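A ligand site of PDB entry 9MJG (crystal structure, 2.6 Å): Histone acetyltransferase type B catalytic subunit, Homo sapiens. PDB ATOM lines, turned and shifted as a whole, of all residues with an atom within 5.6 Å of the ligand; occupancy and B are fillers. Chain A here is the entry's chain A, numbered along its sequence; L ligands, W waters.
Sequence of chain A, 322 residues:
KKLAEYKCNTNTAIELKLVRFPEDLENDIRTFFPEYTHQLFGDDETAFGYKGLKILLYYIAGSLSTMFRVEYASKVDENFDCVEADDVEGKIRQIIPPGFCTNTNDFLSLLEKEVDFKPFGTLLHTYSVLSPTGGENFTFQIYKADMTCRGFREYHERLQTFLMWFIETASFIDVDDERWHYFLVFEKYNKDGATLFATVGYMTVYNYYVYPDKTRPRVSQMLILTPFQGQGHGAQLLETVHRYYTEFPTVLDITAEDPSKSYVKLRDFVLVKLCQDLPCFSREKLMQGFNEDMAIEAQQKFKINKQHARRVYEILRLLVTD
Water W2 lies within hydrogen-bond range of O4 of the ligand, N of Ala 235 and N of Gly 234. Water W1 lies within hydrogen-bond range of the side-chain hydroxyl (OG) of Ser 262 (3.1 Å) and an oxygen (O3) of the ligand (3.3 Å).
An oxygen (O6) of the ligand sits at hydrogen-bond distance from the backbone NH (N) of Gly 230 (2.5 Å). The backbone NH of Gly 234 lies within hydrogen-bond range of an oxygen (O5) of the ligand (2.9 Å). The backbone NH (N) of Ile 224 sits at hydrogen-bond distance from an oxygen (O2) of the ligand (2.9 Å). A nitrogen (N1) of the ligand sits at hydrogen-bond distance from the backbone carbonyl oxygen of Met 222 (3.0 Å). The side-chain hydroxyl of Ser 262 sits close to an oxygen (O3) of the ligand.
CG1 of Val 219 touches F1 of the ligand (3.1 Å). Leu 223 touches the ligand (CA to O2, 3.6 Å). Gln 229 touches the ligand. N of Gly 232 touches O4 of the ligand, 3.98 Å away. His 233 touches the ligand (N to O4, 3.5 Å). Ala 256 touches the ligand (CB to F1, 3.5 Å). CD1 of Tyr 263 touches F1 of the ligand (3.2 Å). Leu 266 touches the ligand. Hydrophobic or aromatic side chains within 4 Å of the ligand: Val 219, Met 222, Leu 223, Ile 224, Ala 256, Tyr 263 and Leu 266. Of the 23 residues printed, 13 come within 4 Å of the ligand. The nearest printed residue that does not touch the ligand is Gln 231 (4.1 Å).
O of Ile 224 is in hydrogen-bond range of NE2 of Gln 229 (3.0 Å). OG of Ser 262 lies within hydrogen-bond range of OG of Ser 260 (3.2 Å). The side-chain hydroxyl (OG) of Ser 260 is in hydrogen-bond range of the backbone NH (N) of Tyr 263. A ring nitrogen (NE2) of His 233 lies within hydrogen-bond range of the side-chain amide oxygen (OE1) of Gln 231, at 2.6 Å.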
ATOM      1  N   PHE A 166     -15.412  -5.141  18.226  1.00  0.00           N
ATOM      2  CA  PHE A 166     -14.098  -5.713  18.491  1.00  0.00           C
ATOM      3  C   PHE A 166     -13.318  -6.049  17.233  1.00  0.00           C
ATOM      4  O   PHE A 166     -12.162  -6.428  17.339  1.00  0.00           O
ATOM      5  CB  PHE A 166     -14.238  -6.953  19.373  1.00  0.00           C
ATOM      6  CG  PHE A 166     -14.745  -6.533  20.745  1.00  0.00           C
ATOM      7  CD1 PHE A 166     -13.877  -5.949  21.660  1.00  0.00           C
ATOM      8  CD2 PHE A 166     -16.100  -6.633  21.070  1.00  0.00           C
ATOM      9  CE1 PHE A 166     -14.350  -5.526  22.886  1.00  0.00           C
ATOM     10  CE2 PHE A 166     -16.556  -6.208  22.297  1.00  0.00           C
ATOM     11  CZ  PHE A 166     -15.675  -5.655  23.203  1.00  0.00           C
ATOM     12  N   ILE A 167     -13.914  -5.917  16.049  1.00  0.00           N
ATOM     13  CA  ILE A 167     -13.174  -6.116  14.817  1.00  0.00           C
ATOM     14  C   ILE A 167     -13.318  -4.874  13.940  1.00  0.00           C
ATOM     15  O   ILE A 167     -14.430  -4.431  13.663  1.00  0.00           O
ATOM     16  CB  ILE A 167     -13.624  -7.421  14.133  1.00  0.00           C
ATOM     17  CG1 ILE A 167     -13.077  -8.619  14.931  1.00  0.00           C
ATOM     18  CG2 ILE A 167     -13.216  -7.461  12.658  1.00  0.00           C
ATOM     19  CD1 ILE A 167     -13.594  -9.946  14.454  1.00  0.00           C
ATOM     20  N   MET A 203     -16.377 -18.632  15.093  1.00  0.00           N
ATOM     21  CA  MET A 203     -15.588 -18.474  13.887  1.00  0.00           C
ATOM     22  C   MET A 203     -16.510 -18.796  12.713  1.00  0.00           C
ATOM     23  O   MET A 203     -17.216 -19.781  12.769  1.00  0.00           O
ATOM     24  CB  MET A 203     -14.380 -19.436  13.907  1.00  0.00           C
ATOM     25  CG  MET A 203     -13.703 -19.608  12.564  1.00  0.00           C
ATOM     26  SD  MET A 203     -12.393 -20.837  12.527  1.00  0.00           S
ATOM     27  CE  MET A 203     -11.128 -19.885  13.363  1.00  0.00           C
ATOM     28  N   VAL A 219     -11.231 -19.153   6.601  1.00  0.00           N
ATOM     29  CA  VAL A 219     -11.662 -18.503   7.820  1.00  0.00           C
ATOM     30  C   VAL A 219     -11.914 -17.029   7.517  1.00  0.00           C
ATOM     31  O   VAL A 219     -11.043 -16.355   6.987  1.00  0.00           O
ATOM     32  CB  VAL A 219     -10.602 -18.672   8.940  1.00  0.00           C
ATOM     33  CG1 VAL A 219     -11.037 -17.982  10.227  1.00  0.00           C
ATOM     34  CG2 VAL A 219     -10.286 -20.136   9.186  1.00  0.00           C
ATOM     35  N   SER A 220     -13.108 -16.544   7.877  1.00  0.00           N
ATOM     36  CA  SER A 220     -13.579 -15.212   7.543  1.00  0.00           C
ATOM     37  C   SER A 220     -13.448 -14.311   8.764  1.00  0.00           C
ATOM     38  O   SER A 220     -12.773 -13.286   8.708  1.00  0.00           O
ATOM     39  CB  SER A 220     -15.009 -15.273   7.075  1.00  0.00           C
ATOM     40  OG  SER A 220     -15.657 -14.015   7.218  1.00  0.00           O
ATOM     41  N   MET A 222     -13.063 -14.538  13.251  1.00  0.00           N
ATOM     42  CA  MET A 222     -12.991 -15.269  14.504  1.00  0.00           C
ATOM     43  C   MET A 222     -13.065 -14.263  15.646  1.00  0.00           C
ATOM     44  O   MET A 222     -12.273 -13.327  15.691  1.00  0.00           O
ATOM     45  CB  MET A 222     -11.699 -16.062  14.649  1.00  0.00           C
ATOM     46  CG  MET A 222     -11.698 -16.970  15.872  1.00  0.00           C
ATOM     47  SD  MET A 222     -10.063 -17.241  16.568  1.00  0.00           S
ATOM     48  CE  MET A 222      -9.507 -18.587  15.533  1.00  0.00           C
ATOM     49  N   LEU A 223     -14.024 -14.470  16.554  1.00  0.00           N
ATOM     50  CA  LEU A 223     -14.174 -13.607  17.713  1.00  0.00           C
ATOM     51  C   LEU A 223     -14.112 -14.429  18.987  1.00  0.00           C
ATOM     52  O   LEU A 223     -14.951 -15.300  19.195  1.00  0.00           O
ATOM     53  CB  LEU A 223     -15.515 -12.879  17.632  1.00  0.00           C
ATOM     54  CG  LEU A 223     -15.876 -12.081  18.876  1.00  0.00           C
ATOM     55  CD1 LEU A 223     -15.070 -10.791  18.899  1.00  0.00           C
ATOM     56  CD2 LEU A 223     -17.359 -11.803  18.893  1.00  0.00           C
ATOM     57  N   ILE A 224     -13.161 -14.103  19.850  1.00  0.00           N
ATOM     58  CA  ILE A 224     -13.153 -14.568  21.236  1.00  0.00           C
ATOM     59  C   ILE A 224     -13.532 -13.379  22.115  1.00  0.00           C
ATOM     60  O   ILE A 224     -12.868 -12.363  22.072  1.00  0.00           O
ATOM     61  CB  ILE A 224     -11.773 -15.149  21.611  1.00  0.00           C
ATOM     62  CG1 ILE A 224     -11.349 -16.240  20.644  1.00  0.00           C
ATOM     63  CG2 ILE A 224     -11.744 -15.637  23.059  1.00  0.00           C
ATOM     64  CD1 ILE A 224     -12.358 -17.385  20.509  1.00  0.00           C
ATOM     65  N   LEU A 225     -14.600 -13.523  22.896  1.00  0.00           N
ATOM     66  CA  LEU A 225     -15.085 -12.404  23.681  1.00  0.00           C
ATOM     67  C   LEU A 225     -14.064 -12.046  24.758  1.00  0.00           C
ATOM     68  O   LEU A 225     -13.359 -12.932  25.278  1.00  0.00           O
ATOM     69  CB  LEU A 225     -16.454 -12.768  24.249  1.00  0.00           C
ATOM     70  CG  LEU A 225     -17.570 -12.995  23.220  1.00  0.00           C
ATOM     71  CD1 LEU A 225     -18.785 -13.670  23.820  1.00  0.00           C
ATOM     72  CD2 LEU A 225     -17.964 -11.665  22.581  1.00  0.00           C
ATOM     73  N   PHE A 228     -12.631 -13.990  27.862  1.00  0.00           N
ATOM     74  CA  PHE A 228     -12.058 -15.309  27.657  1.00  0.00           C
ATOM     75  C   PHE A 228     -10.755 -15.248  26.864  1.00  0.00           C
ATOM     76  O   PHE A 228     -10.243 -16.268  26.403  1.00  0.00           O
ATOM     77  CB  PHE A 228     -13.063 -16.205  26.936  1.00  0.00           C
ATOM     78  CG  PHE A 228     -14.440 -16.198  27.592  1.00  0.00           C
ATOM     79  CD1 PHE A 228     -15.363 -15.223  27.237  1.00  0.00           C
ATOM     80  CD2 PHE A 228     -14.804 -17.161  28.536  1.00  0.00           C
ATOM     81  CE1 PHE A 228     -16.625 -15.198  27.842  1.00  0.00           C
ATOM     82  CE2 PHE A 228     -16.034 -17.099  29.164  1.00  0.00           C
ATOM     83  CZ  PHE A 228     -16.950 -16.132  28.810  1.00  0.00           C
ATOM     84  N   GLN A 229     -10.184 -14.046  26.714  1.00  0.00           N
ATOM     85  CA  GLN A 229      -8.960 -13.917  25.940  1.00  0.00           C
ATOM     86  C   GLN A 229      -7.769 -14.313  26.789  1.00  0.00           C
ATOM     87  O   GLN A 229      -7.770 -14.107  28.002  1.00  0.00           O
ATOM     88  CB  GLN A 229      -8.856 -12.497  25.395  1.00  0.00           C
ATOM     89  CG  GLN A 229      -9.940 -12.170  24.387  1.00  0.00           C
ATOM     90  CD  GLN A 229      -9.699 -10.904  23.623  1.00  0.00           C
ATOM     91  OE1 GLN A 229      -8.848 -10.081  24.000  1.00  0.00           O
ATOM     92  NE2 GLN A 229     -10.446 -10.728  22.543  1.00  0.00           N
ATOM     93  N   GLY A 230      -6.782 -14.940  26.142  1.00  0.00           N
ATOM     94  CA  GLY A 230      -5.533 -15.324  26.783  1.00  0.00           C
ATOM     95  C   GLY A 230      -5.660 -16.679  27.469  1.00  0.00           C
ATOM     96  O   GLY A 230      -5.026 -16.910  28.489  1.00  0.00           O
ATOM     97  N   GLN A 231      -6.492 -17.563  26.921  1.00  0.00           N
ATOM     98  CA  GLN A 231      -6.771 -18.871  27.476  1.00  0.00           C
ATOM     99  C   GLN A 231      -6.510 -19.978  26.460  1.00  0.00           C
ATOM    100  O   GLN A 231      -6.556 -21.150  26.820  1.00  0.00           O
ATOM    101  CB  GLN A 231      -8.244 -18.928  27.889  1.00  0.00           C
ATOM    102  CG  GLN A 231      -8.626 -17.964  29.001  1.00  0.00           C
ATOM    103  CD  GLN A 231     -10.061 -18.130  29.464  1.00  0.00           C
ATOM    104  OE1 GLN A 231     -10.885 -18.831  28.865  1.00  0.00           O
ATOM    105  NE2 GLN A 231     -10.396 -17.440  30.556  1.00  0.00           N
ATOM    106  N   GLY A 232      -6.306 -19.607  25.181  1.00  0.00           N
ATOM    107  CA  GLY A 232      -5.943 -20.534  24.120  1.00  0.00           C
ATOM    108  C   GLY A 232      -7.136 -20.982  23.294  1.00  0.00           C
ATOM    109  O   GLY A 232      -7.062 -21.999  22.632  1.00  0.00           O
ATOM    110  N   HIS A 233      -8.244 -20.239  23.320  1.00  0.00           N
ATOM    111  CA  HIS A 233      -9.458 -20.662  22.639  1.00  0.00           C
ATOM    112  C   HIS A 233      -9.285 -20.647  21.114  1.00  0.00           C
ATOM    113  O   HIS A 233      -9.755 -21.555  20.436  1.00  0.00           O
ATOM    114  CB  HIS A 233     -10.661 -19.834  23.097  1.00  0.00           C
ATOM    115  CG  HIS A 233     -10.995 -20.103  24.522  1.00  0.00           C
ATOM    116  ND1 HIS A 233     -11.146 -21.385  24.999  1.00  0.00           N
ATOM    117  CD2 HIS A 233     -11.170 -19.291  25.567  1.00  0.00           C
ATOM    118  CE1 HIS A 233     -11.428 -21.332  26.282  1.00  0.00           C
ATOM    119  NE2 HIS A 233     -11.430 -20.075  26.660  1.00  0.00           N
ATOM    120  N   GLY A 234      -8.584 -19.656  20.585  1.00  0.00           N
ATOM    121  CA  GLY A 234      -8.372 -19.584  19.146  1.00  0.00           C
ATOM    122  C   GLY A 234      -7.570 -20.769  18.637  1.00  0.00           C
ATOM    123  O   GLY A 234      -7.873 -21.308  17.563  1.00  0.00           O
ATOM    124  N   ALA A 235      -6.571 -21.201  19.414  1.00  0.00           N
ATOM    125  CA  ALA A 235      -5.751 -22.351  19.048  1.00  0.00           C
ATOM    126  C   ALA A 235      -6.593 -23.624  19.004  1.00  0.00           C
ATOM    127  O   ALA A 235      -6.433 -24.448  18.101  1.00  0.00           O
ATOM    128  CB  ALA A 235      -4.596 -22.487  20.006  1.00  0.00           C
ATOM    129  N   ALA A 256      -6.974 -18.485   5.564  1.00  0.00           N
ATOM    130  CA  ALA A 256      -7.699 -17.336   6.086  1.00  0.00           C
ATOM    131  C   ALA A 256      -7.891 -16.305   4.984  1.00  0.00           C
ATOM    132  O   ALA A 256      -6.984 -16.092   4.212  1.00  0.00           O
ATOM    133  CB  ALA A 256      -6.970 -16.716   7.274  1.00  0.00           C
ATOM    134  N   ASP A 258      -8.069 -13.169   5.644  1.00  0.00           N
ATOM    135  CA  ASP A 258      -7.403 -11.968   6.107  1.00  0.00           C
ATOM    136  C   ASP A 258      -6.233 -12.346   7.009  1.00  0.00           C
ATOM    137  O   ASP A 258      -6.329 -12.264   8.221  1.00  0.00           O
ATOM    138  CB  ASP A 258      -8.431 -11.064   6.768  1.00  0.00           C
ATOM    139  CG  ASP A 258      -9.445 -10.460   5.795  1.00  0.00           C
ATOM    140  OD1 ASP A 258      -9.206 -10.543   4.574  1.00  0.00           O
ATOM    141  OD2 ASP A 258     -10.481  -9.936   6.259  1.00  0.00           O
ATOM    142  N   SER A 260      -3.798 -11.657   9.073  1.00  0.00           N
ATOM    143  CA  SER A 260      -3.200 -10.686   9.978  1.00  0.00           C
ATOM    144  C   SER A 260      -1.937 -11.254  10.629  1.00  0.00           C
ATOM    145  O   SER A 260      -1.652 -12.442  10.511  1.00  0.00           O
ATOM    146  CB  SER A 260      -4.173 -10.260  11.023  1.00  0.00           C
ATOM    147  OG  SER A 260      -4.610 -11.362  11.797  1.00  0.00           O
ATOM    148  N   SER A 262      -1.688 -11.566  13.773  1.00  0.00           N
ATOM    149  CA  SER A 262      -2.142 -12.417  14.860  1.00  0.00           C
ATOM    150  C   SER A 262      -2.630 -13.770  14.333  1.00  0.00           C
ATOM    151  O   SER A 262      -2.374 -14.795  14.963  1.00  0.00           O
ATOM    152  CB  SER A 262      -3.151 -11.719  15.742  1.00  0.00           C
ATOM    153  OG  SER A 262      -4.291 -11.319  14.999  1.00  0.00           O
ATOM    154  N   TYR A 263      -3.280 -13.774  13.160  1.00  0.00           N
ATOM    155  CA  TYR A 263      -3.643 -15.005  12.481  1.00  0.00           C
ATOM    156  C   TYR A 263      -2.403 -15.857  12.201  1.00  0.00           C
ATOM    157  O   TYR A 263      -2.405 -17.057  12.433  1.00  0.00           O
ATOM    158  CB  TYR A 263      -4.372 -14.825  11.138  1.00  0.00           C
ATOM    159  CG  TYR A 263      -4.355 -16.086  10.283  1.00  0.00           C
ATOM    160  CD1 TYR A 263      -5.196 -17.156  10.565  1.00  0.00           C
ATOM    161  CD2 TYR A 263      -3.485 -16.220   9.206  1.00  0.00           C
ATOM    162  CE1 TYR A 263      -5.173 -18.317   9.809  1.00  0.00           C
ATOM    163  CE2 TYR A 263      -3.452 -17.361   8.428  1.00  0.00           C
ATOM    164  CZ  TYR A 263      -4.298 -18.418   8.730  1.00  0.00           C
ATOM    165  OH  TYR A 263      -4.279 -19.555   7.971  1.00  0.00           O
ATOM    166  N   LEU A 266      -1.099 -17.405  15.276  1.00  0.00           N
ATOM    167  CA  LEU A 266      -1.986 -18.465  15.687  1.00  0.00           C
ATOM    168  C   LEU A 266      -1.806 -19.675  14.770  1.00  0.00           C
ATOM    169  O   LEU A 266      -1.722 -20.792  15.249  1.00  0.00           O
ATOM    170  CB  LEU A 266      -3.427 -17.968  15.663  1.00  0.00           C
ATOM    171  CG  LEU A 266      -4.492 -19.018  15.957  1.00  0.00           C
ATOM    172  CD1 LEU A 266      -4.220 -19.642  17.306  1.00  0.00           C
ATOM    173  CD2 LEU A 266      -5.842 -18.382  15.954  1.00  0.00           C
HETATM  174  C1  LIG L   1      -6.702 -12.897  22.570  1.00  0.00           C
HETATM  175  C2  LIG L   1      -7.011 -12.147  21.448  1.00  0.00           C
HETATM  176  C3  LIG L   1      -7.551 -12.737  20.312  1.00  0.00           C
HETATM  177  C4  LIG L   1      -7.931 -11.807  19.158  1.00  0.00           C
HETATM  178  C5  LIG L   1      -9.251 -11.043  19.399  1.00  0.00           C
HETATM  179  C6  LIG L   1      -7.881 -12.402  17.777  1.00  0.00           C
HETATM  180  C7  LIG L   1      -7.789 -13.888  15.405  1.00  0.00           C
HETATM  181  C8  LIG L   1      -8.011 -14.559  11.640  1.00  0.00           C
HETATM  182  C9  LIG L   1      -8.174 -15.930  11.693  1.00  0.00           C
HETATM  183  C10 LIG L   1      -7.969 -15.946  14.033  1.00  0.00           C
HETATM  184  C11 LIG L   1      -7.775 -14.114  20.293  1.00  0.00           C
HETATM  185  C12 LIG L   1      -4.932 -10.927  25.088  1.00  0.00           C
HETATM  186  C13 LIG L   1      -5.559 -11.094  23.725  1.00  0.00           C
HETATM  187  O1  LIG L   1      -6.146 -12.392  23.709  1.00  0.00           O
HETATM  188  C14 LIG L   1     -10.441 -11.680  18.746  1.00  0.00           C
HETATM  189  O2  LIG L   1     -11.544 -11.768  19.282  1.00  0.00           O
HETATM  190  N1  LIG L   1     -10.223 -12.177  17.501  1.00  0.00           N
HETATM  191  C15 LIG L   1      -9.016 -12.663  17.078  1.00  0.00           C
HETATM  192  C16 LIG L   1      -6.587 -12.667  17.175  1.00  0.00           C
HETATM  193  O3  LIG L   1      -5.555 -12.389  17.767  1.00  0.00           O
HETATM  194  C17 LIG L   1      -6.522 -13.287  15.806  1.00  0.00           C
HETATM  195  C18 LIG L   1      -7.798 -14.565  14.052  1.00  0.00           C
HETATM  196  C19 LIG L   1      -7.825 -13.881  12.837  1.00  0.00           C
HETATM  197  F1  LIG L   1      -8.309 -16.621  10.532  1.00  0.00           F
HETATM  198  C20 LIG L   1      -8.156 -16.634  12.858  1.00  0.00           C
HETATM  199  C21 LIG L   1      -8.905 -12.927  15.612  1.00  0.00           C
HETATM  200  C22 LIG L   1      -7.467 -14.875  21.437  1.00  0.00           C
HETATM  201  N2  LIG L   1      -7.632 -16.348  21.363  1.00  0.00           N
HETATM  202  O4  LIG L   1      -7.199 -17.033  22.280  1.00  0.00           O
HETATM  203  O5  LIG L   1      -8.138 -16.829  20.372  1.00  0.00           O
HETATM  204  C23 LIG L   1      -6.924 -14.278  22.595  1.00  0.00           C
HETATM  205  O6  LIG L   1      -6.542 -14.990  23.687  1.00  0.00           O
HETATM  206  O   HOH W   1      -6.775  -9.809  16.211  1.00  0.00           O
HETATM  207  O   HOH W   2      -5.553 -18.895  21.218  1.00  0.00           O
